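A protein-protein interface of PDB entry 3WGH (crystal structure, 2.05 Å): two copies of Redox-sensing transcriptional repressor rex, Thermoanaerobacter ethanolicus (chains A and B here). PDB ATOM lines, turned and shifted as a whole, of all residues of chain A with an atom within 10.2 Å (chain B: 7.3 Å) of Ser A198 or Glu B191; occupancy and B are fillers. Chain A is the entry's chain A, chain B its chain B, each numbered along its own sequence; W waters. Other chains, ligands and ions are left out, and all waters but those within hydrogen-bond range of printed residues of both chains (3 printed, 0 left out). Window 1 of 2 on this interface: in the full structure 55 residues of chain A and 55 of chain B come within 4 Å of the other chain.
Ser A198 touches just these residues of chain B: Trp B175 (2.8 Å), Glu B191 (2.6 Å) and Val B193 (3.7 Å). Glu B191 touches just these residues of chain A: Ser A198 (2.6 Å), Thr A201 (3.6 Å), Val A202 (3.5 Å) and Arg A205 (2.7 Å). No residue of chain A comes within 4 Å of Asn B192. Printed residues of chain A within 4 Å of Ala B173: Val A202. Of the printed residues of chain A, Pro B16 touches Asp A197. Val B188 touches none of the printed residues of chain A. The nearest residue of chain A that does not touch Glu B191 is Leu A199 (5.2 Å).
The side-chain hydroxyl of Thr A201 lies within hydrogen-bond range of the backbone carbonyl oxygen of Ser A198. O of Ile B174 sits at hydrogen-bond distance from N of Glu B191 (2.9 Å). The side-chain hydroxyl (OG1) of Thr A201 is in hydrogen-bond range of the guanidinium group (NH2) of Arg A205 (2.8 Å). The backbone carbonyl oxygen (O) of Asn B176 sits at hydrogen-bond distance from the backbone NH (N) of Val B193 (2.8 Å). N of Ile B174 is in hydrogen-bond range of O of Ile B189 (2.7 Å). The backbone carbonyl oxygen (O) of Ala B173 is in hydrogen-bond range of the backbone NH (N) of Gly B150, 3.0 Å away.
CZ2 of Trp B175 touches O of Leu A195 (3.5 Å). CG1 of Val B193 touches CD2 of Leu A195 (3.9 Å). Asp A197 touches Pro B16. CG2 of Val B193 touches OG of Ser A198, 3.7 Å away. CB of Leu A199 touches CZ2 of Trp B175, 3.7 Å away. CG2 of Thr A201 touches NH1 of Arg B13, 3.8 Å away. Val A202 touches Ala B173 (CG1 to CB, 3.7 Å). Met B9 touches Arg A205 (CE to CZ, 3.8 Å). Arg A205 touches Ile B189. Ile B189 touches Leu A206.
Water W1 lies within hydrogen-bond range of a ring nitrogen (ND1) of His B194 (2.5 Å), the backbone carbonyl oxygen of Asn B192 (3.3 Å) and the guanidinium group of Arg A20 (3.5 Å). Water W2 lies within hydrogen-bond range of the backbone carbonyl oxygen (O) of Asp A197 (2.8 Å) and the guanidinium group (NH1) of Arg B13 (3.0 Å). Water W3 lies within hydrogen-bond range of NH1 of Arg A205, O of Leu B190 and OE1 of Glu B191.
Of the 17 printed residues of chain B, 10 touch a printed residue of chain A. Hydrophobic or aromatic side chains of chain B within 4 Å of the printed part of chain A: Met B9, Pro B16, Ala B173, Trp B175, Ile B189, Val B193 and His B194. Of the 17 printed residues of chain A, 9 touch a printed residue of chain B. Hydrophobic or aromatic side chains of chain A within 4 Å of the printed part of chain B: Leu A195, Leu A199, Val A202 and Leu A206. Along chain A the printed residues that touch a printed residue of chain B span positions 20 to 206.
The side-chain hydroxyl of Ser A198 is in hydrogen-bond range of the indole nitrogen of Trp B175, 2.8 Å away. The side-chain hydroxyl (OG) of Ser A198 lies within hydrogen-bond range of the side-chain carboxylate (OE2) of Glu B191 (2.6 Å). ND1 of His B194 lies close to NH2 of Arg A20 (3.5 Å). NH2 of Arg A205 is in salt-bridge range of OE1 of Glu B191, at 2.7 Å.
Positions printed for both chains: 193 and 194. Of the 17 pairs that touch across the chains among the printed residues, none has its exchanged pair printed and touching as well.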
ATOM      1  N   ARG A  17     -23.427  16.003  -7.287  1.00  0.00           N
ATOM      2  CA  ARG A  17     -22.926  16.980  -6.395  1.00  0.00           C
ATOM      3  C   ARG A  17     -23.968  17.372  -5.325  1.00  0.00           C
ATOM      4  O   ARG A  17     -23.623  17.512  -4.145  1.00  0.00           O
ATOM      5  CB  ARG A  17     -22.383  18.174  -7.174  1.00  0.00           C
ATOM      6  CG  ARG A  17     -21.566  19.048  -6.234  1.00  0.00           C
ATOM      7  CD  ARG A  17     -20.748  20.171  -6.942  1.00  0.00           C
ATOM      8  NE  ARG A  17     -20.112  20.988  -5.902  1.00  0.00           N
ATOM      9  CZ  ARG A  17     -20.568  22.171  -5.475  1.00  0.00           C
ATOM     10  NH1 ARG A  17     -21.634  22.720  -6.043  1.00  0.00           N
ATOM     11  NH2 ARG A  17     -19.961  22.788  -4.466  1.00  0.00           N
ATOM     12  N   ARG A  20     -23.887  14.269  -3.001  1.00  0.00           N
ATOM     13  CA  ARG A  20     -22.718  14.399  -2.053  1.00  0.00           C
ATOM     14  C   ARG A  20     -22.951  15.338  -0.875  1.00  0.00           C
ATOM     15  O   ARG A  20     -22.604  15.061   0.269  1.00  0.00           O
ATOM     16  CB  ARG A  20     -21.429  14.849  -2.786  1.00  0.00           C
ATOM     17  CG  ARG A  20     -20.732  13.712  -3.502  1.00  0.00           C
ATOM     18  CD  ARG A  20     -19.296  14.169  -3.922  1.00  0.00           C
ATOM     19  NE  ARG A  20     -19.239  15.140  -5.042  1.00  0.00           N
ATOM     20  CZ  ARG A  20     -18.987  16.437  -4.924  1.00  0.00           C
ATOM     21  NH1 ARG A  20     -18.756  16.988  -3.724  1.00  0.00           N
ATOM     22  NH2 ARG A  20     -18.872  17.168  -6.033  1.00  0.00           N
ATOM     23  N   TYR A  21     -23.468  16.510  -1.153  1.00  0.00           N
ATOM     24  CA  TYR A  21     -23.676  17.443  -0.117  1.00  0.00           C
ATOM     25  C   TYR A  21     -24.765  17.014   0.852  1.00  0.00           C
ATOM     26  O   TYR A  21     -24.631  17.198   2.052  1.00  0.00           O
ATOM     27  CB  TYR A  21     -23.958  18.815  -0.683  1.00  0.00           C
ATOM     28  CG  TYR A  21     -22.655  19.572  -0.856  1.00  0.00           C
ATOM     29  CD1 TYR A  21     -22.201  20.462   0.141  1.00  0.00           C
ATOM     30  CD2 TYR A  21     -21.824  19.337  -1.967  1.00  0.00           C
ATOM     31  CE1 TYR A  21     -20.986  21.141   0.007  1.00  0.00           C
ATOM     32  CE2 TYR A  21     -20.596  20.014  -2.098  1.00  0.00           C
ATOM     33  CZ  TYR A  21     -20.191  20.902  -1.105  1.00  0.00           C
ATOM     34  OH  TYR A  21     -18.980  21.551  -1.237  1.00  0.00           O
ATOM     35  N   VAL A 193     -13.909  10.571 -18.809  1.00  0.00           N
ATOM     36  CA  VAL A 193     -13.356  11.292 -17.674  1.00  0.00           C
ATOM     37  C   VAL A 193     -12.225  12.233 -18.159  1.00  0.00           C
ATOM     38  O   VAL A 193     -11.376  11.825 -18.932  1.00  0.00           O
ATOM     39  CB  VAL A 193     -12.772  10.297 -16.632  1.00  0.00           C
ATOM     40  CG1 VAL A 193     -12.120  11.053 -15.442  1.00  0.00           C
ATOM     41  CG2 VAL A 193     -13.850   9.299 -16.187  1.00  0.00           C
ATOM     42  N   HIS A 194     -12.221  13.479 -17.710  1.00  0.00           N
ATOM     43  CA  HIS A 194     -11.064  14.369 -17.996  1.00  0.00           C
ATOM     44  C   HIS A 194     -10.613  15.000 -16.691  1.00  0.00           C
ATOM     45  O   HIS A 194     -11.204  15.994 -16.234  1.00  0.00           O
ATOM     46  CB  HIS A 194     -11.459  15.479 -18.995  1.00  0.00           C
ATOM     47  CG  HIS A 194     -11.909  14.944 -20.314  1.00  0.00           C
ATOM     48  ND1 HIS A 194     -13.240  14.755 -20.626  1.00  0.00           N
ATOM     49  CD2 HIS A 194     -11.200  14.508 -21.388  1.00  0.00           C
ATOM     50  CE1 HIS A 194     -13.335  14.227 -21.836  1.00  0.00           C
ATOM     51  NE2 HIS A 194     -12.112  14.069 -22.315  1.00  0.00           N
ATOM     52  N   LEU A 195      -9.586  14.431 -16.074  1.00  0.00           N
ATOM     53  CA  LEU A 195      -9.088  15.032 -14.816  1.00  0.00           C
ATOM     54  C   LEU A 195      -8.590  16.476 -15.032  1.00  0.00           C
ATOM     55  O   LEU A 195      -8.586  17.266 -14.124  1.00  0.00           O
ATOM     56  CB  LEU A 195      -7.978  14.188 -14.172  1.00  0.00           C
ATOM     57  CG  LEU A 195      -8.548  12.908 -13.527  1.00  0.00           C
ATOM     58  CD1 LEU A 195      -7.366  12.021 -13.082  1.00  0.00           C
ATOM     59  CD2 LEU A 195      -9.499  13.222 -12.379  1.00  0.00           C
ATOM     60  N   SER A 196      -8.220  16.800 -16.257  1.00  0.00           N
ATOM     61  CA  SER A 196      -7.738  18.163 -16.566  1.00  0.00           C
ATOM     62  C   SER A 196      -8.809  19.243 -16.303  1.00  0.00           C
ATOM     63  O   SER A 196      -8.472  20.366 -15.912  1.00  0.00           O
ATOM     64  CB  SER A 196      -7.204  18.209 -18.001  1.00  0.00           C
ATOM     65  OG  SER A 196      -8.224  18.005 -18.952  1.00  0.00           O
ATOM     66  N   ASP A 197     -10.086  18.869 -16.398  1.00  0.00           N
ATOM     67  CA  ASP A 197     -11.179  19.797 -16.131  1.00  0.00           C
ATOM     68  C   ASP A 197     -11.113  20.218 -14.655  1.00  0.00           C
ATOM     69  O   ASP A 197     -11.589  21.309 -14.298  1.00  0.00           O
ATOM     70  CB  ASP A 197     -12.582  19.192 -16.358  1.00  0.00           C
ATOM     71  CG  ASP A 197     -12.952  18.961 -17.870  1.00  0.00           C
ATOM     72  OD1 ASP A 197     -12.180  19.288 -18.785  1.00  0.00           O
ATOM     73  OD2 ASP A 197     -14.066  18.420 -18.118  1.00  0.00           O
ATOM     74  N   SER A 198     -10.601  19.356 -13.776  1.00  0.00           N
ATOM     75  CA  SER A 198     -10.488  19.748 -12.335  1.00  0.00           C
ATOM     76  C   SER A 198      -9.134  20.497 -12.148  1.00  0.00           C
ATOM     77  O   SER A 198      -9.040  21.558 -11.514  1.00  0.00           O
ATOM     78  CB  SER A 198     -10.547  18.478 -11.435  1.00  0.00           C
ATOM     79  OG  SER A 198     -10.161  18.811 -10.096  1.00  0.00           O
ATOM     80  N   LEU A 199      -8.077  19.994 -12.777  1.00  0.00           N
ATOM     81  CA  LEU A 199      -6.752  20.593 -12.529  1.00  0.00           C
ATOM     82  C   LEU A 199      -6.692  22.009 -13.088  1.00  0.00           C
ATOM     83  O   LEU A 199      -6.091  22.884 -12.469  1.00  0.00           O
ATOM     84  CB  LEU A 199      -5.646  19.744 -13.202  1.00  0.00           C
ATOM     85  CG  LEU A 199      -4.204  20.277 -13.113  1.00  0.00           C
ATOM     86  CD1 LEU A 199      -3.702  20.374 -11.669  1.00  0.00           C
ATOM     87  CD2 LEU A 199      -3.244  19.464 -13.998  1.00  0.00           C
ATOM     88  N   PHE A 200      -7.268  22.226 -14.276  1.00  0.00           N
ATOM     89  CA  PHE A 200      -7.118  23.525 -14.920  1.00  0.00           C
ATOM     90  C   PHE A 200      -7.886  24.578 -14.109  1.00  0.00           C
ATOM     91  O   PHE A 200      -7.677  25.755 -14.331  1.00  0.00           O
ATOM     92  CB  PHE A 200      -7.606  23.499 -16.363  1.00  0.00           C
ATOM     93  CG  PHE A 200      -6.731  22.709 -17.326  1.00  0.00           C
ATOM     94  CD1 PHE A 200      -5.485  22.169 -16.940  1.00  0.00           C
ATOM     95  CD2 PHE A 200      -7.161  22.506 -18.603  1.00  0.00           C
ATOM     96  CE1 PHE A 200      -4.674  21.444 -17.855  1.00  0.00           C
ATOM     97  CE2 PHE A 200      -6.335  21.832 -19.567  1.00  0.00           C
ATOM     98  CZ  PHE A 200      -5.110  21.271 -19.183  1.00  0.00           C
ATOM     99  N   THR A 201      -8.763  24.194 -13.150  1.00  0.00           N
ATOM    100  CA  THR A 201      -9.378  25.241 -12.301  1.00  0.00           C
ATOM    101  C   THR A 201      -8.404  25.661 -11.194  1.00  0.00           C
ATOM    102  O   THR A 201      -8.622  26.651 -10.515  1.00  0.00           O
ATOM    103  CB  THR A 201     -10.738  24.792 -11.540  1.00  0.00           C
ATOM    104  OG1 THR A 201     -10.435  23.805 -10.551  1.00  0.00           O
ATOM    105  CG2 THR A 201     -11.779  24.210 -12.517  1.00  0.00           C
ATOM    106  N   VAL A 202      -7.371  24.855 -10.952  1.00  0.00           N
ATOM    107  CA  VAL A 202      -6.332  25.243  -9.955  1.00  0.00           C
ATOM    108  C   VAL A 202      -5.367  26.245 -10.574  1.00  0.00           C
ATOM    109  O   VAL A 202      -5.066  27.228  -9.955  1.00  0.00           O
ATOM    110  CB  VAL A 202      -5.488  24.024  -9.480  1.00  0.00           C
ATOM    111  CG1 VAL A 202      -4.398  24.512  -8.519  1.00  0.00           C
ATOM    112  CG2 VAL A 202      -6.471  22.985  -8.830  1.00  0.00           C
ATOM    113  N   SER A 203      -4.934  26.000 -11.799  1.00  0.00           N
ATOM    114  CA  SER A 203      -4.170  27.055 -12.484  1.00  0.00           C
ATOM    115  C   SER A 203      -4.992  28.349 -12.711  1.00  0.00           C
ATOM    116  O   SER A 203      -4.431  29.419 -12.695  1.00  0.00           O
ATOM    117  CB  SER A 203      -3.554  26.546 -13.801  1.00  0.00           C
ATOM    118  OG  SER A 203      -4.544  25.956 -14.623  1.00  0.00           O
ATOM    119  N   TYR A 204      -6.306  28.228 -12.993  1.00  0.00           N
ATOM    120  CA  TYR A 204      -7.134  29.433 -13.156  1.00  0.00           C
ATOM    121  C   TYR A 204      -7.097  30.207 -11.841  1.00  0.00           C
ATOM    122  O   TYR A 204      -6.833  31.419 -11.836  1.00  0.00           O
ATOM    123  CB  TYR A 204      -8.580  29.083 -13.586  1.00  0.00           C
ATOM    124  CG  TYR A 204      -9.457  30.305 -13.554  1.00  0.00           C
ATOM    125  CD1 TYR A 204      -9.975  30.764 -12.328  1.00  0.00           C
ATOM    126  CD2 TYR A 204      -9.555  31.161 -14.694  1.00  0.00           C
ATOM    127  CE1 TYR A 204     -10.697  31.952 -12.246  1.00  0.00           C
ATOM    128  CE2 TYR A 204     -10.256  32.371 -14.610  1.00  0.00           C
ATOM    129  CZ  TYR A 204     -10.839  32.744 -13.398  1.00  0.00           C
ATOM    130  OH  TYR A 204     -11.514  33.936 -13.307  1.00  0.00           O
ATOM    131  N   ARG A 205      -7.400  29.535 -10.702  1.00  0.00           N
ATOM    132  CA  ARG A 205      -7.430  30.244  -9.421  1.00  0.00           C
ATOM    133  C   ARG A 205      -6.087  30.845  -8.978  1.00  0.00           C
ATOM    134  O   ARG A 205      -6.030  31.985  -8.522  1.00  0.00           O
ATOM    135  CB  ARG A 205      -8.031  29.362  -8.318  1.00  0.00           C
ATOM    136  CG  ARG A 205      -9.591  29.345  -8.437  1.00  0.00           C
ATOM    137  CD  ARG A 205     -10.180  28.306  -7.410  1.00  0.00           C
ATOM    138  NE  ARG A 205     -10.122  26.952  -7.994  1.00  0.00           N
ATOM    139  CZ  ARG A 205     -10.627  25.886  -7.351  1.00  0.00           C
ATOM    140  NH1 ARG A 205     -11.094  26.068  -6.114  1.00  0.00           N
ATOM    141  NH2 ARG A 205     -10.650  24.681  -7.899  1.00  0.00           N
ATOM    142  N   LEU A 206      -5.014  30.104  -9.139  1.00  0.00           N
ATOM    143  CA  LEU A 206      -3.681  30.667  -8.808  1.00  0.00           C
ATOM    144  C   LEU A 206      -3.350  31.934  -9.648  1.00  0.00           C
ATOM    145  O   LEU A 206      -2.767  32.885  -9.144  1.00  0.00           O
ATOM    146  CB  LEU A 206      -2.585  29.612  -9.049  1.00  0.00           C
ATOM    147  CG  LEU A 206      -2.547  28.425  -8.061  1.00  0.00           C
ATOM    148  CD1 LEU A 206      -1.612  27.330  -8.592  1.00  0.00           C
ATOM    149  CD2 LEU A 206      -2.065  28.989  -6.722  1.00  0.00           C
ATOM    150  N   MET B   9     -17.416  30.204  -9.326  1.00  0.00           N
ATOM    151  CA  MET B   9     -16.979  28.813  -9.572  1.00  0.00           C
ATOM    152  C   MET B   9     -17.772  28.152 -10.669  1.00  0.00           C
ATOM    153  O   MET B   9     -17.197  27.403 -11.460  1.00  0.00           O
ATOM    154  CB  MET B   9     -17.052  27.952  -8.297  1.00  0.00           C
ATOM    155  CG  MET B   9     -15.844  28.144  -7.395  1.00  0.00           C
ATOM    156  SD  MET B   9     -14.231  28.006  -8.245  1.00  0.00           S
ATOM    157  CE  MET B   9     -14.118  26.355  -8.897  1.00  0.00           C
ATOM    158  N   ARG B  13     -15.718  26.500 -13.688  1.00  0.00           N
ATOM    159  CA  ARG B  13     -15.814  25.078 -14.019  1.00  0.00           C
ATOM    160  C   ARG B  13     -16.241  24.785 -15.446  1.00  0.00           C
ATOM    161  O   ARG B  13     -15.879  23.756 -15.970  1.00  0.00           O
ATOM    162  CB  ARG B  13     -16.707  24.305 -13.020  1.00  0.00           C
ATOM    163  CG  ARG B  13     -16.057  24.232 -11.632  1.00  0.00           C
ATOM    164  CD  ARG B  13     -16.545  23.036 -10.809  1.00  0.00           C
ATOM    165  NE  ARG B  13     -15.957  23.037  -9.453  1.00  0.00           N
ATOM    166  CZ  ARG B  13     -14.769  22.538  -9.129  1.00  0.00           C
ATOM    167  NH1 ARG B  13     -13.891  22.129 -10.077  1.00  0.00           N
ATOM    168  NH2 ARG B  13     -14.390  22.600  -7.872  1.00  0.00           N
ATOM    169  N   PRO B  16     -12.645  25.023 -18.510  1.00  0.00           N
ATOM    170  CA  PRO B  16     -11.844  23.954 -19.077  1.00  0.00           C
ATOM    171  C   PRO B  16     -12.597  23.103 -20.094  1.00  0.00           C
ATOM    172  O   PRO B  16     -11.950  22.577 -21.010  1.00  0.00           O
ATOM    173  CB  PRO B  16     -11.437  23.114 -17.841  1.00  0.00           C
ATOM    174  CG  PRO B  16     -11.585  24.104 -16.684  1.00  0.00           C
ATOM    175  CD  PRO B  16     -12.819  24.866 -17.057  1.00  0.00           C
ATOM    176  N   GLY B 150       0.513  20.828  -4.412  1.00  0.00           N
ATOM    177  CA  GLY B 150       0.641  19.449  -3.907  1.00  0.00           C
ATOM    178  C   GLY B 150      -0.573  18.586  -4.327  1.00  0.00           C
ATOM    179  O   GLY B 150      -1.736  18.972  -4.137  1.00  0.00           O
ATOM    180  N   ALA B 173      -1.537  25.516  -3.229  1.00  0.00           N
ATOM    181  CA  ALA B 173      -2.752  24.806  -3.683  1.00  0.00           C
ATOM    182  C   ALA B 173      -2.611  23.327  -3.409  1.00  0.00           C
ATOM    183  O   ALA B 173      -1.513  22.795  -3.513  1.00  0.00           O
ATOM    184  CB  ALA B 173      -2.928  25.024  -5.209  1.00  0.00           C
ATOM    185  N   ILE B 174      -3.735  22.662  -3.147  1.00  0.00           N
ATOM    186  CA  ILE B 174      -3.783  21.213  -2.966  1.00  0.00           C
ATOM    187  C   ILE B 174      -4.802  20.645  -3.955  1.00  0.00           C
ATOM    188  O   ILE B 174      -5.976  21.029  -3.962  1.00  0.00           O
ATOM    189  CB  ILE B 174      -4.173  20.833  -1.493  1.00  0.00           C
ATOM    190  CG1 ILE B 174      -3.057  21.311  -0.529  1.00  0.00           C
ATOM    191  CG2 ILE B 174      -4.324  19.319  -1.375  1.00  0.00           C
ATOM    192  CD1 ILE B 174      -3.247  20.876   0.937  1.00  0.00           C
ATOM    193  N   TRP B 175      -4.342  19.725  -4.804  1.00  0.00           N
ATOM    194  CA  TRP B 175      -5.255  18.939  -5.658  1.00  0.00           C
ATOM    195  C   TRP B 175      -5.538  17.627  -4.940  1.00  0.00           C
ATOM    196  O   TRP B 175      -4.682  16.787  -4.845  1.00  0.00           O
ATOM    197  CB  TRP B 175      -4.633  18.726  -7.061  1.00  0.00           C
ATOM    198  CG  TRP B 175      -5.630  18.330  -8.124  1.00  0.00           C
ATOM    199  CD1 TRP B 175      -6.993  18.600  -8.152  1.00  0.00           C
ATOM    200  CD2 TRP B 175      -5.346  17.577  -9.313  1.00  0.00           C
ATOM    201  NE1 TRP B 175      -7.540  18.118  -9.314  1.00  0.00           N
ATOM    202  CE2 TRP B 175      -6.574  17.441 -10.027  1.00  0.00           C
ATOM    203  CE3 TRP B 175      -4.176  17.042  -9.853  1.00  0.00           C
ATOM    204  CZ2 TRP B 175      -6.669  16.763 -11.228  1.00  0.00           C
ATOM    205  CZ3 TRP B 175      -4.260  16.331 -11.062  1.00  0.00           C
ATOM    206  CH2 TRP B 175      -5.507  16.219 -11.751  1.00  0.00           C
ATOM    207  N   ASN B 176      -6.716  17.511  -4.334  1.00  0.00           N
ATOM    208  CA  ASN B 176      -6.958  16.474  -3.348  1.00  0.00           C
ATOM    209  C   ASN B 176      -7.826  15.347  -3.952  1.00  0.00           C
ATOM    210  O   ASN B 176      -8.931  15.619  -4.422  1.00  0.00           O
ATOM    211  CB  ASN B 176      -7.677  17.071  -2.123  1.00  0.00           C
ATOM    212  CG  ASN B 176      -8.174  15.953  -1.172  1.00  0.00           C
ATOM    213  OD1 ASN B 176      -7.444  14.991  -0.935  1.00  0.00           O
ATOM    214  ND2 ASN B 176      -9.427  16.020  -0.752  1.00  0.00           N
ATOM    215  N   PHE B 177      -7.319  14.113  -3.988  1.00  0.00           N
ATOM    216  CA  PHE B 177      -8.113  12.970  -4.396  1.00  0.00           C
ATOM    217  C   PHE B 177      -8.776  12.246  -3.222  1.00  0.00           C
ATOM    218  O   PHE B 177      -9.563  11.322  -3.423  1.00  0.00           O
ATOM    219  CB  PHE B 177      -7.247  11.973  -5.196  1.00  0.00           C
ATOM    220  CG  PHE B 177      -6.917  12.458  -6.569  1.00  0.00           C
ATOM    221  CD1 PHE B 177      -7.680  12.053  -7.663  1.00  0.00           C
ATOM    222  CD2 PHE B 177      -5.899  13.418  -6.753  1.00  0.00           C
ATOM    223  CE1 PHE B 177      -7.392  12.593  -8.993  1.00  0.00           C
ATOM    224  CE2 PHE B 177      -5.555  13.883  -8.045  1.00  0.00           C
ATOM    225  CZ  PHE B 177      -6.308  13.494  -9.152  1.00  0.00           C
ATOM    226  N   LEU B 178      -8.468  12.611  -1.995  1.00  0.00           N
ATOM    227  CA  LEU B 178      -9.048  11.780  -0.915  1.00  0.00           C
ATOM    228  C   LEU B 178     -10.502  12.076  -0.668  1.00  0.00           C
ATOM    229  O   LEU B 178     -10.898  13.221  -0.667  1.00  0.00           O
ATOM    230  CB  LEU B 178      -8.290  11.899   0.394  1.00  0.00           C
ATOM    231  CG  LEU B 178      -6.794  12.134   0.468  1.00  0.00           C
ATOM    232  CD1 LEU B 178      -6.344  11.604   1.794  1.00  0.00           C
ATOM    233  CD2 LEU B 178      -5.929  11.632  -0.704  1.00  0.00           C
ATOM    234  N   VAL B 188      -5.355  29.296   0.725  1.00  0.00           N
ATOM    235  CA  VAL B 188      -4.818  28.131   0.012  1.00  0.00           C
ATOM    236  C   VAL B 188      -5.909  27.550  -0.853  1.00  0.00           C
ATOM    237  O   VAL B 188      -7.040  27.432  -0.389  1.00  0.00           O
ATOM    238  CB  VAL B 188      -4.320  27.045   0.997  1.00  0.00           C
ATOM    239  CG1 VAL B 188      -3.952  25.738   0.254  1.00  0.00           C
ATOM    240  CG2 VAL B 188      -3.103  27.554   1.805  1.00  0.00           C
ATOM    241  N   ILE B 189      -5.612  27.272  -2.134  1.00  0.00           N
ATOM    242  CA  ILE B 189      -6.605  26.691  -3.035  1.00  0.00           C
ATOM    243  C   ILE B 189      -6.745  25.196  -2.789  1.00  0.00           C
ATOM    244  O   ILE B 189      -5.762  24.460  -2.781  1.00  0.00           O
ATOM    245  CB  ILE B 189      -6.249  26.988  -4.525  1.00  0.00           C
ATOM    246  CG1 ILE B 189      -6.337  28.521  -4.760  1.00  0.00           C
ATOM    247  CG2 ILE B 189      -7.236  26.201  -5.516  1.00  0.00           C
ATOM    248  CD1 ILE B 189      -5.408  28.967  -5.823  1.00  0.00           C
ATOM    249  N   LEU B 190      -7.960  24.738  -2.503  1.00  0.00           N
ATOM    250  CA  LEU B 190      -8.165  23.306  -2.326  1.00  0.00           C
ATOM    251  C   LEU B 190      -9.129  22.850  -3.447  1.00  0.00           C
ATOM    252  O   LEU B 190     -10.258  23.376  -3.542  1.00  0.00           O
ATOM    253  CB  LEU B 190      -8.819  23.074  -0.979  1.00  0.00           C
ATOM    254  CG  LEU B 190      -9.281  21.652  -0.655  1.00  0.00           C
ATOM    255  CD1 LEU B 190      -8.139  20.630  -0.699  1.00  0.00           C
ATOM    256  CD2 LEU B 190     -10.024  21.617   0.694  1.00  0.00           C
ATOM    257  N   GLU B 191      -8.703  21.937  -4.307  1.00  0.00           N
ATOM    258  CA  GLU B 191      -9.586  21.432  -5.351  1.00  0.00           C
ATOM    259  C   GLU B 191      -9.818  19.942  -5.071  1.00  0.00           C
ATOM    260  O   GLU B 191      -8.873  19.150  -5.059  1.00  0.00           O
ATOM    261  CB  GLU B 191      -8.970  21.645  -6.752  1.00  0.00           C
ATOM    262  CG  GLU B 191      -9.646  20.848  -7.924  1.00  0.00           C
ATOM    263  CD  GLU B 191     -11.137  21.234  -8.194  1.00  0.00           C
ATOM    264  OE1 GLU B 191     -11.654  22.159  -7.528  1.00  0.00           O
ATOM    265  OE2 GLU B 191     -11.798  20.637  -9.097  1.00  0.00           O
ATOM    266  N   ASN B 192     -11.061  19.556  -4.799  1.00  0.00           N
ATOM    267  CA  ASN B 192     -11.309  18.151  -4.432  1.00  0.00           C
ATOM    268  C   ASN B 192     -11.768  17.374  -5.648  1.00  0.00           C
ATOM    269  O   ASN B 192     -12.598  17.868  -6.413  1.00  0.00           O
ATOM    270  CB  ASN B 192     -12.377  18.083  -3.386  1.00  0.00           C
ATOM    271  CG  ASN B 192     -11.939  18.701  -2.088  1.00  0.00           C
ATOM    272  OD1 ASN B 192     -10.902  18.320  -1.536  1.00  0.00           O
ATOM    273  ND2 ASN B 192     -12.747  19.662  -1.572  1.00  0.00           N
ATOM    274  N   VAL B 193     -11.212  16.178  -5.869  1.00  0.00           N
ATOM    275  CA  VAL B 193     -11.654  15.372  -7.029  1.00  0.00           C
ATOM    276  C   VAL B 193     -12.730  14.392  -6.530  1.00  0.00           C
ATOM    277  O   VAL B 193     -12.503  13.703  -5.531  1.00  0.00           O
ATOM    278  CB  VAL B 193     -10.512  14.611  -7.733  1.00  0.00           C
ATOM    279  CG1 VAL B 193     -11.115  13.660  -8.857  1.00  0.00           C
ATOM    280  CG2 VAL B 193      -9.507  15.619  -8.396  1.00  0.00           C
ATOM    281  N   HIS B 194     -13.848  14.277  -7.242  1.00  0.00           N
ATOM    282  CA  HIS B 194     -14.832  13.172  -6.987  1.00  0.00           C
ATOM    283  C   HIS B 194     -15.135  12.466  -8.274  1.00  0.00           C
ATOM    284  O   HIS B 194     -16.034  12.903  -9.016  1.00  0.00           O
ATOM    285  CB  HIS B 194     -16.168  13.706  -6.445  1.00  0.00           C
ATOM    286  CG  HIS B 194     -15.999  14.579  -5.238  1.00  0.00           C
ATOM    287  ND1 HIS B 194     -15.725  15.922  -5.339  1.00  0.00           N
ATOM    288  CD2 HIS B 194     -15.939  14.281  -3.922  1.00  0.00           C
ATOM    289  CE1 HIS B 194     -15.565  16.427  -4.134  1.00  0.00           C
ATOM    290  NE2 HIS B 194     -15.678  15.450  -3.269  1.00  0.00           N
HETATM  291  O   HOH W   1     -15.695  17.311  -7.407  1.00  0.00           O
HETATM  292  O   HOH W   2     -14.017  21.252 -12.901  1.00  0.00           O
HETATM  293  O   HOH W   3     -12.883  24.057  -4.956  1.00  0.00           O
